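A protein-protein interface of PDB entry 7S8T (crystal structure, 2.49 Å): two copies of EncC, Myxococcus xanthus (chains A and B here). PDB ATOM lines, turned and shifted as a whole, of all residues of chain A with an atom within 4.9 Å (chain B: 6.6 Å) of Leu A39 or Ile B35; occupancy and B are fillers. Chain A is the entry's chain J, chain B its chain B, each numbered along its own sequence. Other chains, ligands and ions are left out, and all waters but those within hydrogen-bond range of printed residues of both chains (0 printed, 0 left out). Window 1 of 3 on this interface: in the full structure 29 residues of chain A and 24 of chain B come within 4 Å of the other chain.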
ATOM      1  N   ILE A  35     -18.793   6.210  27.322  1.00  0.00           N
ATOM      2  CA  ILE A  35     -17.670   7.089  27.633  1.00  0.00           C
ATOM      3  C   ILE A  35     -18.184   8.448  28.083  1.00  0.00           C
ATOM      4  O   ILE A  35     -17.731   9.002  29.091  1.00  0.00           O
ATOM      5  CB  ILE A  35     -16.734   7.232  26.418  1.00  0.00           C
ATOM      6  CG1 ILE A  35     -16.160   5.884  25.998  1.00  0.00           C
ATOM      7  CG2 ILE A  35     -15.597   8.194  26.737  1.00  0.00           C
ATOM      8  CD1 ILE A  35     -15.601   5.877  24.596  1.00  0.00           C
ATOM      9  N   GLU A  36     -19.156   8.995  27.346  1.00  0.00           N
ATOM     10  CA  GLU A  36     -19.739  10.281  27.721  1.00  0.00           C
ATOM     11  C   GLU A  36     -20.330  10.238  29.126  1.00  0.00           C
ATOM     12  O   GLU A  36     -20.127  11.160  29.926  1.00  0.00           O
ATOM     13  CB  GLU A  36     -20.818  10.682  26.714  1.00  0.00           C
ATOM     14  CG  GLU A  36     -20.322  10.970  25.311  1.00  0.00           C
ATOM     15  CD  GLU A  36     -21.467  11.167  24.335  1.00  0.00           C
ATOM     16  OE1 GLU A  36     -21.329  11.975  23.398  1.00  0.00           O
ATOM     17  OE2 GLU A  36     -22.516  10.512  24.515  1.00  0.00           O
ATOM     18  N   ALA A  37     -21.058   9.166  29.444  1.00  0.00           N
ATOM     19  CA  ALA A  37     -21.714   9.081  30.747  1.00  0.00           C
ATOM     20  C   ALA A  37     -20.699   8.980  31.880  1.00  0.00           C
ATOM     21  O   ALA A  37     -20.845   9.643  32.916  1.00  0.00           O
ATOM     22  CB  ALA A  37     -22.667   7.886  30.777  1.00  0.00           C
ATOM     23  N   GLU A  38     -19.665   8.161  31.676  1.00  0.00           N
ATOM     24  CA  GLU A  38     -18.592   8.042  32.697  1.00  0.00           C
ATOM     25  C   GLU A  38     -17.965   9.421  32.907  1.00  0.00           C
ATOM     26  O   GLU A  38     -17.810   9.824  34.076  1.00  0.00           O
ATOM     27  CB  GLU A  38     -17.538   7.032  32.241  1.00  0.00           C
ATOM     28  CG  GLU A  38     -18.071   5.614  32.134  1.00  0.00           C
ATOM     29  CD  GLU A  38     -18.654   5.073  33.427  1.00  0.00           C
ATOM     30  OE1 GLU A  38     -18.066   5.338  34.494  1.00  0.00           O
ATOM     31  OE2 GLU A  38     -19.692   4.386  33.364  1.00  0.00           O
ATOM     32  N   LEU A  39     -17.643  10.119  31.815  1.00  0.00           N
ATOM     33  CA  LEU A  39     -16.987  11.419  31.922  1.00  0.00           C
ATOM     34  C   LEU A  39     -17.850  12.421  32.677  1.00  0.00           C
ATOM     35  O   LEU A  39     -17.344  13.184  33.506  1.00  0.00           O
ATOM     36  CB  LEU A  39     -16.657  11.949  30.527  1.00  0.00           C
ATOM     37  CG  LEU A  39     -15.687  11.129  29.680  1.00  0.00           C
ATOM     38  CD1 LEU A  39     -15.344  11.882  28.416  1.00  0.00           C
ATOM     39  CD2 LEU A  39     -14.435  10.801  30.468  1.00  0.00           C
ATOM     40  N   ASP A  40     -19.160  12.423  32.421  1.00  0.00           N
ATOM     41  CA  ASP A  40     -20.038  13.330  33.159  1.00  0.00           C
ATOM     42  C   ASP A  40     -20.077  12.976  34.642  1.00  0.00           C
ATOM     43  O   ASP A  40     -20.120  13.866  35.501  1.00  0.00           O
ATOM     44  CB  ASP A  40     -21.445  13.324  32.564  1.00  0.00           C
ATOM     45  CG  ASP A  40     -22.213  14.593  32.886  1.00  0.00           C
ATOM     46  OD1 ASP A  40     -21.644  15.692  32.703  1.00  0.00           O
ATOM     47  OD2 ASP A  40     -23.376  14.493  33.324  1.00  0.00           O
ATOM     48  N   ALA A  41     -20.079  11.681  34.965  1.00  0.00           N
ATOM     49  CA  ALA A  41     -20.072  11.284  36.370  1.00  0.00           C
ATOM     50  C   ALA A  41     -18.792  11.740  37.066  1.00  0.00           C
ATOM     51  O   ALA A  41     -18.830  12.229  38.208  1.00  0.00           O
ATOM     52  CB  ALA A  41     -20.251   9.772  36.482  1.00  0.00           C
ATOM     53  N   ILE A  42     -17.647  11.597  36.391  1.00  0.00           N
ATOM     54  CA  ILE A  42     -16.392  12.078  36.964  1.00  0.00           C
ATOM     55  C   ILE A  42     -16.456  13.589  37.146  1.00  0.00           C
ATOM     56  O   ILE A  42     -15.925  14.135  38.117  1.00  0.00           O
ATOM     57  CB  ILE A  42     -15.184  11.656  36.107  1.00  0.00           C
ATOM     58  CG1 ILE A  42     -15.200  10.153  35.842  1.00  0.00           C
ATOM     59  CG2 ILE A  42     -13.887  11.993  36.822  1.00  0.00           C
ATOM     60  CD1 ILE A  42     -14.441   9.758  34.591  1.00  0.00           C
ATOM     61  N   ASN A  43     -17.096  14.287  36.203  1.00  0.00           N
ATOM     62  CA  ASN A  43     -17.253  15.733  36.332  1.00  0.00           C
ATOM     63  C   ASN A  43     -18.049  16.090  37.582  1.00  0.00           C
ATOM     64  O   ASN A  43     -17.698  17.029  38.306  1.00  0.00           O
ATOM     65  CB  ASN A  43     -17.953  16.301  35.095  1.00  0.00           C
ATOM     66  CG  ASN A  43     -16.994  16.618  33.975  1.00  0.00           C
ATOM     67  OD1 ASN A  43     -15.821  16.266  34.040  1.00  0.00           O
ATOM     68  ND2 ASN A  43     -17.484  17.298  32.946  1.00  0.00           N
ATOM     69  N   ALA A  72     -13.648   5.241  32.409  1.00  0.00           N
ATOM     70  CA  ALA A  72     -13.556   6.045  31.197  1.00  0.00           C
ATOM     71  C   ALA A  72     -12.355   5.629  30.364  1.00  0.00           C
ATOM     72  O   ALA A  72     -12.448   5.515  29.137  1.00  0.00           O
ATOM     73  CB  ALA A  72     -13.471   7.530  31.552  1.00  0.00           C
ATOM     74  N   TRP A  76     -12.566   3.967  26.680  1.00  0.00           N
ATOM     75  CA  TRP A  76     -11.817   4.659  25.643  1.00  0.00           C
ATOM     76  C   TRP A  76     -10.894   3.711  24.893  1.00  0.00           C
ATOM     77  O   TRP A  76     -10.843   3.719  23.657  1.00  0.00           O
ATOM     78  CB  TRP A  76     -11.001   5.778  26.277  1.00  0.00           C
ATOM     79  CG  TRP A  76     -10.299   6.558  25.273  1.00  0.00           C
ATOM     80  CD1 TRP A  76      -9.016   6.394  24.848  1.00  0.00           C
ATOM     81  CD2 TRP A  76     -10.843   7.631  24.519  1.00  0.00           C
ATOM     82  NE1 TRP A  76      -8.727   7.310  23.872  1.00  0.00           N
ATOM     83  CE2 TRP A  76      -9.835   8.088  23.656  1.00  0.00           C
ATOM     84  CE3 TRP A  76     -12.090   8.257  24.496  1.00  0.00           C
ATOM     85  CZ2 TRP A  76     -10.034   9.144  22.776  1.00  0.00           C
ATOM     86  CZ3 TRP A  76     -12.286   9.300  23.628  1.00  0.00           C
ATOM     87  CH2 TRP A  76     -11.265   9.736  22.778  1.00  0.00           C
ATOM     88  N   ARG B  29     -13.438  19.548  34.448  1.00  0.00           N
ATOM     89  CA  ARG B  29     -14.807  19.170  34.125  1.00  0.00           C
ATOM     90  C   ARG B  29     -15.191  19.648  32.733  1.00  0.00           C
ATOM     91  O   ARG B  29     -15.842  18.922  31.969  1.00  0.00           O
ATOM     92  CB  ARG B  29     -15.764  19.780  35.151  1.00  0.00           C
ATOM     93  CG  ARG B  29     -15.922  19.039  36.460  1.00  0.00           C
ATOM     94  CD  ARG B  29     -16.719  19.895  37.442  1.00  0.00           C
ATOM     95  NE  ARG B  29     -18.158  19.670  37.327  1.00  0.00           N
ATOM     96  CZ  ARG B  29     -18.965  20.367  36.533  1.00  0.00           C
ATOM     97  NH1 ARG B  29     -18.482  21.345  35.779  1.00  0.00           N
ATOM     98  NH2 ARG B  29     -20.262  20.088  36.493  1.00  0.00           N
ATOM     99  N   SER B  30     -14.759  20.856  32.375  1.00  0.00           N
ATOM    100  CA  SER B  30     -15.087  21.420  31.072  1.00  0.00           C
ATOM    101  C   SER B  30     -14.445  20.641  29.934  1.00  0.00           C
ATOM    102  O   SER B  30     -15.066  20.444  28.884  1.00  0.00           O
ATOM    103  CB  SER B  30     -14.654  22.881  31.027  1.00  0.00           C
ATOM    104  OG  SER B  30     -13.243  22.984  30.944  1.00  0.00           O
ATOM    105  N   ILE B  31     -13.211  20.175  30.116  1.00  0.00           N
ATOM    106  CA  ILE B  31     -12.561  19.447  29.035  1.00  0.00           C
ATOM    107  C   ILE B  31     -13.156  18.050  28.900  1.00  0.00           C
ATOM    108  O   ILE B  31     -13.329  17.542  27.785  1.00  0.00           O
ATOM    109  CB  ILE B  31     -11.036  19.413  29.250  1.00  0.00           C
ATOM    110  CG1 ILE B  31     -10.460  20.831  29.182  1.00  0.00           C
ATOM    111  CG2 ILE B  31     -10.364  18.518  28.221  1.00  0.00           C
ATOM    112  CD1 ILE B  31     -10.814  21.586  27.918  1.00  0.00           C
ATOM    113  N   ARG B  32     -13.517  17.418  30.020  1.00  0.00           N
ATOM    114  CA  ARG B  32     -14.265  16.163  29.917  1.00  0.00           C
ATOM    115  C   ARG B  32     -15.586  16.367  29.173  1.00  0.00           C
ATOM    116  O   ARG B  32     -15.984  15.532  28.348  1.00  0.00           O
ATOM    117  CB  ARG B  32     -14.498  15.581  31.310  1.00  0.00           C
ATOM    118  CG  ARG B  32     -13.210  15.225  32.049  1.00  0.00           C
ATOM    119  CD  ARG B  32     -13.494  14.453  33.326  1.00  0.00           C
ATOM    120  NE  ARG B  32     -12.493  14.708  34.356  1.00  0.00           N
ATOM    121  CZ  ARG B  32     -12.788  15.008  35.618  1.00  0.00           C
ATOM    122  NH1 ARG B  32     -14.054  15.112  35.990  1.00  0.00           N
ATOM    123  NH2 ARG B  32     -11.823  15.224  36.502  1.00  0.00           N
ATOM    124  N   LEU B  33     -16.277  17.481  29.442  1.00  0.00           N
ATOM    125  CA  LEU B  33     -17.515  17.777  28.722  1.00  0.00           C
ATOM    126  C   LEU B  33     -17.265  17.980  27.231  1.00  0.00           C
ATOM    127  O   LEU B  33     -18.071  17.560  26.393  1.00  0.00           O
ATOM    128  CB  LEU B  33     -18.188  19.015  29.316  1.00  0.00           C
ATOM    129  CG  LEU B  33     -19.498  19.415  28.631  1.00  0.00           C
ATOM    130  CD1 LEU B  33     -20.625  18.505  29.083  1.00  0.00           C
ATOM    131  CD2 LEU B  33     -19.847  20.874  28.888  1.00  0.00           C
ATOM    132  N   ASN B  34     -16.163  18.640  26.881  1.00  0.00           N
ATOM    133  CA  ASN B  34     -15.843  18.834  25.471  1.00  0.00           C
ATOM    134  C   ASN B  34     -15.564  17.499  24.793  1.00  0.00           C
ATOM    135  O   ASN B  34     -15.911  17.305  23.619  1.00  0.00           O
ATOM    136  CB  ASN B  34     -14.647  19.773  25.327  1.00  0.00           C
ATOM    137  CG  ASN B  34     -15.001  21.201  25.645  1.00  0.00           C
ATOM    138  OD1 ASN B  34     -16.156  21.513  25.931  1.00  0.00           O
ATOM    139  ND2 ASN B  34     -14.011  22.083  25.598  1.00  0.00           N
ATOM    140  N   ILE B  35     -14.921  16.577  25.518  1.00  0.00           N
ATOM    141  CA  ILE B  35     -14.720  15.222  25.010  1.00  0.00           C
ATOM    142  C   ILE B  35     -16.067  14.565  24.740  1.00  0.00           C
ATOM    143  O   ILE B  35     -16.270  13.924  23.698  1.00  0.00           O
ATOM    144  CB  ILE B  35     -13.877  14.397  26.004  1.00  0.00           C
ATOM    145  CG1 ILE B  35     -12.505  15.024  26.198  1.00  0.00           C
ATOM    146  CG2 ILE B  35     -13.641  12.999  25.481  1.00  0.00           C
ATOM    147  CD1 ILE B  35     -11.696  14.425  27.332  1.00  0.00           C
ATOM    148  N   GLU B  36     -17.010  14.718  25.673  1.00  0.00           N
ATOM    149  CA  GLU B  36     -18.357  14.189  25.471  1.00  0.00           C
ATOM    150  C   GLU B  36     -19.000  14.771  24.214  1.00  0.00           C
ATOM    151  O   GLU B  36     -19.617  14.046  23.428  1.00  0.00           O
ATOM    152  CB  GLU B  36     -19.231  14.486  26.691  1.00  0.00           C
ATOM    153  CG  GLU B  36     -18.809  13.790  27.972  1.00  0.00           C
ATOM    154  CD  GLU B  36     -19.576  14.304  29.177  1.00  0.00           C
ATOM    155  OE1 GLU B  36     -20.776  14.615  29.023  1.00  0.00           O
ATOM    156  OE2 GLU B  36     -18.984  14.396  30.273  1.00  0.00           O
ATOM    157  N   ALA B  37     -18.859  16.082  24.011  1.00  0.00           N
ATOM    158  CA  ALA B  37     -19.491  16.731  22.863  1.00  0.00           C
ATOM    159  C   ALA B  37     -18.888  16.250  21.548  1.00  0.00           C
ATOM    160  O   ALA B  37     -19.613  15.990  20.577  1.00  0.00           O
ATOM    161  CB  ALA B  37     -19.363  18.249  22.984  1.00  0.00           C
ATOM    162  N   GLU B  38     -17.565  16.114  21.499  1.00  0.00           N
ATOM    163  CA  GLU B  38     -16.925  15.602  20.292  1.00  0.00           C
ATOM    164  C   GLU B  38     -17.363  14.170  20.011  1.00  0.00           C
ATOM    165  O   GLU B  38     -17.592  13.797  18.854  1.00  0.00           O
ATOM    166  CB  GLU B  38     -15.405  15.690  20.420  1.00  0.00           C
ATOM    167  CG  GLU B  38     -14.855  17.101  20.304  1.00  0.00           C
ATOM    168  CD  GLU B  38     -15.301  17.794  19.032  1.00  0.00           C
ATOM    169  OE1 GLU B  38     -14.614  17.632  18.004  1.00  0.00           O
ATOM    170  OE2 GLU B  38     -16.316  18.521  19.065  1.00  0.00           O
ATOM    171  N   LEU B  39     -17.480  13.350  21.058  1.00  0.00           N
ATOM    172  CA  LEU B  39     -17.954  11.982  20.873  1.00  0.00           C
ATOM    173  C   LEU B  39     -19.392  11.955  20.366  1.00  0.00           C
ATOM    174  O   LEU B  39     -19.754  11.100  19.550  1.00  0.00           O
ATOM    175  CB  LEU B  39     -17.833  11.204  22.181  1.00  0.00           C
ATOM    176  CG  LEU B  39     -16.428  10.708  22.516  1.00  0.00           C
ATOM    177  CD1 LEU B  39     -16.496   9.667  23.611  1.00  0.00           C
ATOM    178  CD2 LEU B  39     -15.745  10.149  21.280  1.00  0.00           C
ATOM    179  N   ASP B  40     -20.232  12.870  20.854  1.00  0.00           N
ATOM    180  CA  ASP B  40     -21.602  12.937  20.354  1.00  0.00           C
ATOM    181  C   ASP B  40     -21.610  13.295  18.876  1.00  0.00           C
ATOM    182  O   ASP B  40     -22.383  12.732  18.094  1.00  0.00           O
ATOM    183  CB  ASP B  40     -22.414  13.957  21.157  1.00  0.00           C
ATOM    184  CG  ASP B  40     -23.912  13.696  21.097  1.00  0.00           C
ATOM    185  OD1 ASP B  40     -24.349  12.599  21.510  1.00  0.00           O
ATOM    186  OD2 ASP B  40     -24.653  14.594  20.644  1.00  0.00           O
ATOM    187  N   ILE B  42     -19.224  12.599  16.738  1.00  0.00           N
ATOM    188  CA  ILE B  42     -18.742  11.422  16.015  1.00  0.00           C
ATOM    189  C   ILE B  42     -19.857  10.396  15.858  1.00  0.00           C
ATOM    190  O   ILE B  42     -20.045   9.819  14.780  1.00  0.00           O
ATOM    191  CB  ILE B  42     -17.520  10.813  16.733  1.00  0.00           C
ATOM    192  CG1 ILE B  42     -16.323  11.761  16.665  1.00  0.00           C
ATOM    193  CG2 ILE B  42     -17.159   9.469  16.127  1.00  0.00           C
ATOM    194  CD1 ILE B  42     -15.374  11.646  17.845  1.00  0.00           C
ATOM    195  N   HIS B  71     -10.042  15.390  17.293  1.00  0.00           N
ATOM    196  CA  HIS B  71     -10.327  16.296  18.436  1.00  0.00           C
ATOM    197  C   HIS B  71     -10.441  15.472  19.722  1.00  0.00           C
ATOM    198  O   HIS B  71      -9.856  15.890  20.741  1.00  0.00           O
ATOM    199  CB  HIS B  71     -11.593  17.123  18.175  1.00  0.00           C
ATOM    200  CG  HIS B  71     -11.635  17.741  16.819  1.00  0.00           C
ATOM    201  ND1 HIS B  71     -12.815  17.928  16.131  1.00  0.00           N
ATOM    202  CD2 HIS B  71     -10.656  18.212  16.020  1.00  0.00           C
ATOM    203  CE1 HIS B  71     -12.564  18.489  14.968  1.00  0.00           C
ATOM    204  NE2 HIS B  71     -11.250  18.668  14.873  1.00  0.00           N
ATOM    205  N   ALA B  72     -11.156  14.343  19.670  1.00  0.00           N
ATOM    206  CA  ALA B  72     -11.358  13.547  20.876  1.00  0.00           C
ATOM    207  C   ALA B  72     -10.037  13.010  21.401  1.00  0.00           C
ATOM    208  O   ALA B  72      -9.781  13.038  22.611  1.00  0.00           O
ATOM    209  CB  ALA B  72     -12.329  12.399  20.590  1.00  0.00           C
ATOM    210  N   PHE B  75      -8.148  16.030  23.025  1.00  0.00           N
ATOM    211  CA  PHE B  75      -8.713  16.365  24.327  1.00  0.00           C
ATOM    212  C   PHE B  75      -8.381  15.300  25.362  1.00  0.00           C
ATOM    213  O   PHE B  75      -8.152  15.615  26.535  1.00  0.00           O
ATOM    214  CB  PHE B  75     -10.226  16.532  24.211  1.00  0.00           C
ATOM    215  CG  PHE B  75     -10.662  17.880  23.728  1.00  0.00           C
ATOM    216  CD1 PHE B  75      -9.807  18.963  23.782  1.00  0.00           C
ATOM    217  CD2 PHE B  75     -11.939  18.065  23.228  1.00  0.00           C
ATOM    218  CE1 PHE B  75     -10.215  20.203  23.339  1.00  0.00           C
ATOM    219  CE2 PHE B  75     -12.349  19.302  22.784  1.00  0.00           C
ATOM    220  CZ  PHE B  75     -11.488  20.372  22.841  1.00  0.00           C
ATOM    221  N   TRP B  76      -8.335  14.033  24.948  1.00  0.00           N
ATOM    222  CA  TRP B  76      -7.987  12.969  25.882  1.00  0.00           C
ATOM    223  C   TRP B  76      -6.546  13.099  26.352  1.00  0.00           C
ATOM    224  O   TRP B  76      -6.258  12.985  27.553  1.00  0.00           O
ATOM    225  CB  TRP B  76      -8.210  11.609  25.220  1.00  0.00           C
ATOM    226  CG  TRP B  76      -7.843  10.456  26.089  1.00  0.00           C
ATOM    227  CD1 TRP B  76      -6.629   9.836  26.166  1.00  0.00           C
ATOM    228  CD2 TRP B  76      -8.700   9.777  27.006  1.00  0.00           C
ATOM    229  NE1 TRP B  76      -6.678   8.811  27.078  1.00  0.00           N
ATOM    230  CE2 TRP B  76      -7.940   8.754  27.608  1.00  0.00           C
ATOM    231  CE3 TRP B  76     -10.037   9.933  27.379  1.00  0.00           C
ATOM    232  CZ2 TRP B  76      -8.474   7.897  28.561  1.00  0.00           C
ATOM    233  CZ3 TRP B  76     -10.564   9.082  28.323  1.00  0.00           C
ATOM    234  CH2 TRP B  76      -9.785   8.075  28.906  1.00  0.00           C
ATOM    235  N   GLU B  77      -5.627  13.383  25.430  1.00  0.00           N
ATOM    236  CA  GLU B  77      -4.240  13.544  25.855  1.00  0.00           C
ATOM    237  C   GLU B  77      -4.066  14.785  26.725  1.00  0.00           C
ATOM    238  O   GLU B  77      -3.283  14.766  27.681  1.00  0.00           O
ATOM    239  CB  GLU B  77      -3.302  13.589  24.648  1.00  0.00           C
ATOM    240  CG  GLU B  77      -1.870  14.019  24.987  1.00  0.00           C
ATOM    241  CD  GLU B  77      -1.247  13.235  26.141  1.00  0.00           C
ATOM    242  OE1 GLU B  77      -1.558  12.035  26.298  1.00  0.00           O
ATOM    243  OE2 GLU B  77      -0.452  13.832  26.902  1.00  0.00           O
ATOM    244  N   ILE B  79      -6.415  16.116  28.808  1.00  0.00           N
ATOM    245  CA  ILE B  79      -6.942  15.866  30.145  1.00  0.00           C
ATOM    246  C   ILE B  79      -6.010  14.925  30.895  1.00  0.00           C
ATOM    247  O   ILE B  79      -5.922  14.976  32.127  1.00  0.00           O
ATOM    248  CB  ILE B  79      -8.393  15.337  30.096  1.00  0.00           C
ATOM    249  CG1 ILE B  79      -8.989  15.306  31.504  1.00  0.00           C
ATOM    250  CG2 ILE B  79      -8.463  13.962  29.469  1.00  0.00           C
ATOM    251  CD1 ILE B  79      -9.180  16.677  32.113  1.00  0.00           C
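ND2 of Asn A43 lies within hydrogen-bond range of O of Arg B29 (2.5 Å).
OE1 of Glu A36 sits close to O of Glu B36.
NH1 of Arg B32 lies within hydrogen-bond range of O of Ile A42.
The side-chain carboxylate of Glu B36 is in hydrogen-bond range of the backbone NH of Asp A40, at 2.9 Å.
OE1 of Glu A36 is in hydrogen-bond range of N of Asp B40 (2.9 Å).
The side-chain amide oxygen (OD1) of Asn A43 lies within hydrogen-bond range of the guanidinium group (NH1) of Arg B32, 2.9 Å away.
The backbone carbonyl oxygen of Leu A39 lies close to the side-chain amide oxygen of Asn A43.
Among the printed residues, merely in contact across the chains: Leu A39 with Glu B36, Ile A35 with Leu B39, Leu A39 with Ile B35, Glu A36 with Leu B39, Trp A76 with Ala B72, Trp A76 with Trp B76, Ala A72 with Trp B76, Leu A39 with Arg B32 and Asn A43 with Leu B33.
Glu A38 touches none of the printed residues of chain B.
Leu A39 touches just these residues of chain B: Arg B32 (3.7 Å), Ile B35 (3.6 Å) and Glu B36 (3.3 Å).
Of the printed residues of chain B, Asn A43 touches Arg B29, Arg B32 and Leu B33.
Of the printed residues of chain A, Arg B32 touches Leu A39 (3.7 Å), Ile A42 (3.0 Å) and Asn A43 (2.9 Å).
Of the printed residues of chain A, Ile B35 touches Leu A39.
Of the printed residues of chain A, Asp B40 touches Glu A36.
The nearest residue of chain A that does not touch Ile B35 is Trp A76 (4.4 Å).
The nearest printed residue of chain A that does not touch Arg B29 is Ile A42 (5.2 Å).
Of the 19 printed residues of chain B, 9 touch a printed residue of chain A.
Hydrophobic or aromatic side chains of chain B that line the printed part of chain A: Ile B35, Leu B39, Ala B72 and Trp B76.
Among the printed residues, 15 pairs touch across the chains.
Ile A35 touches Leu B39, and with the chains exchanged Leu A39 touches Ile B35.
Glu A36 touches Leu B39, and with the chains exchanged Leu A39 touches Glu B36.
Ala A72 touches Trp B76, and with the chains exchanged Trp A76 touches Ala B72.
Trp B76 touches its own counterpart, Trp A76.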
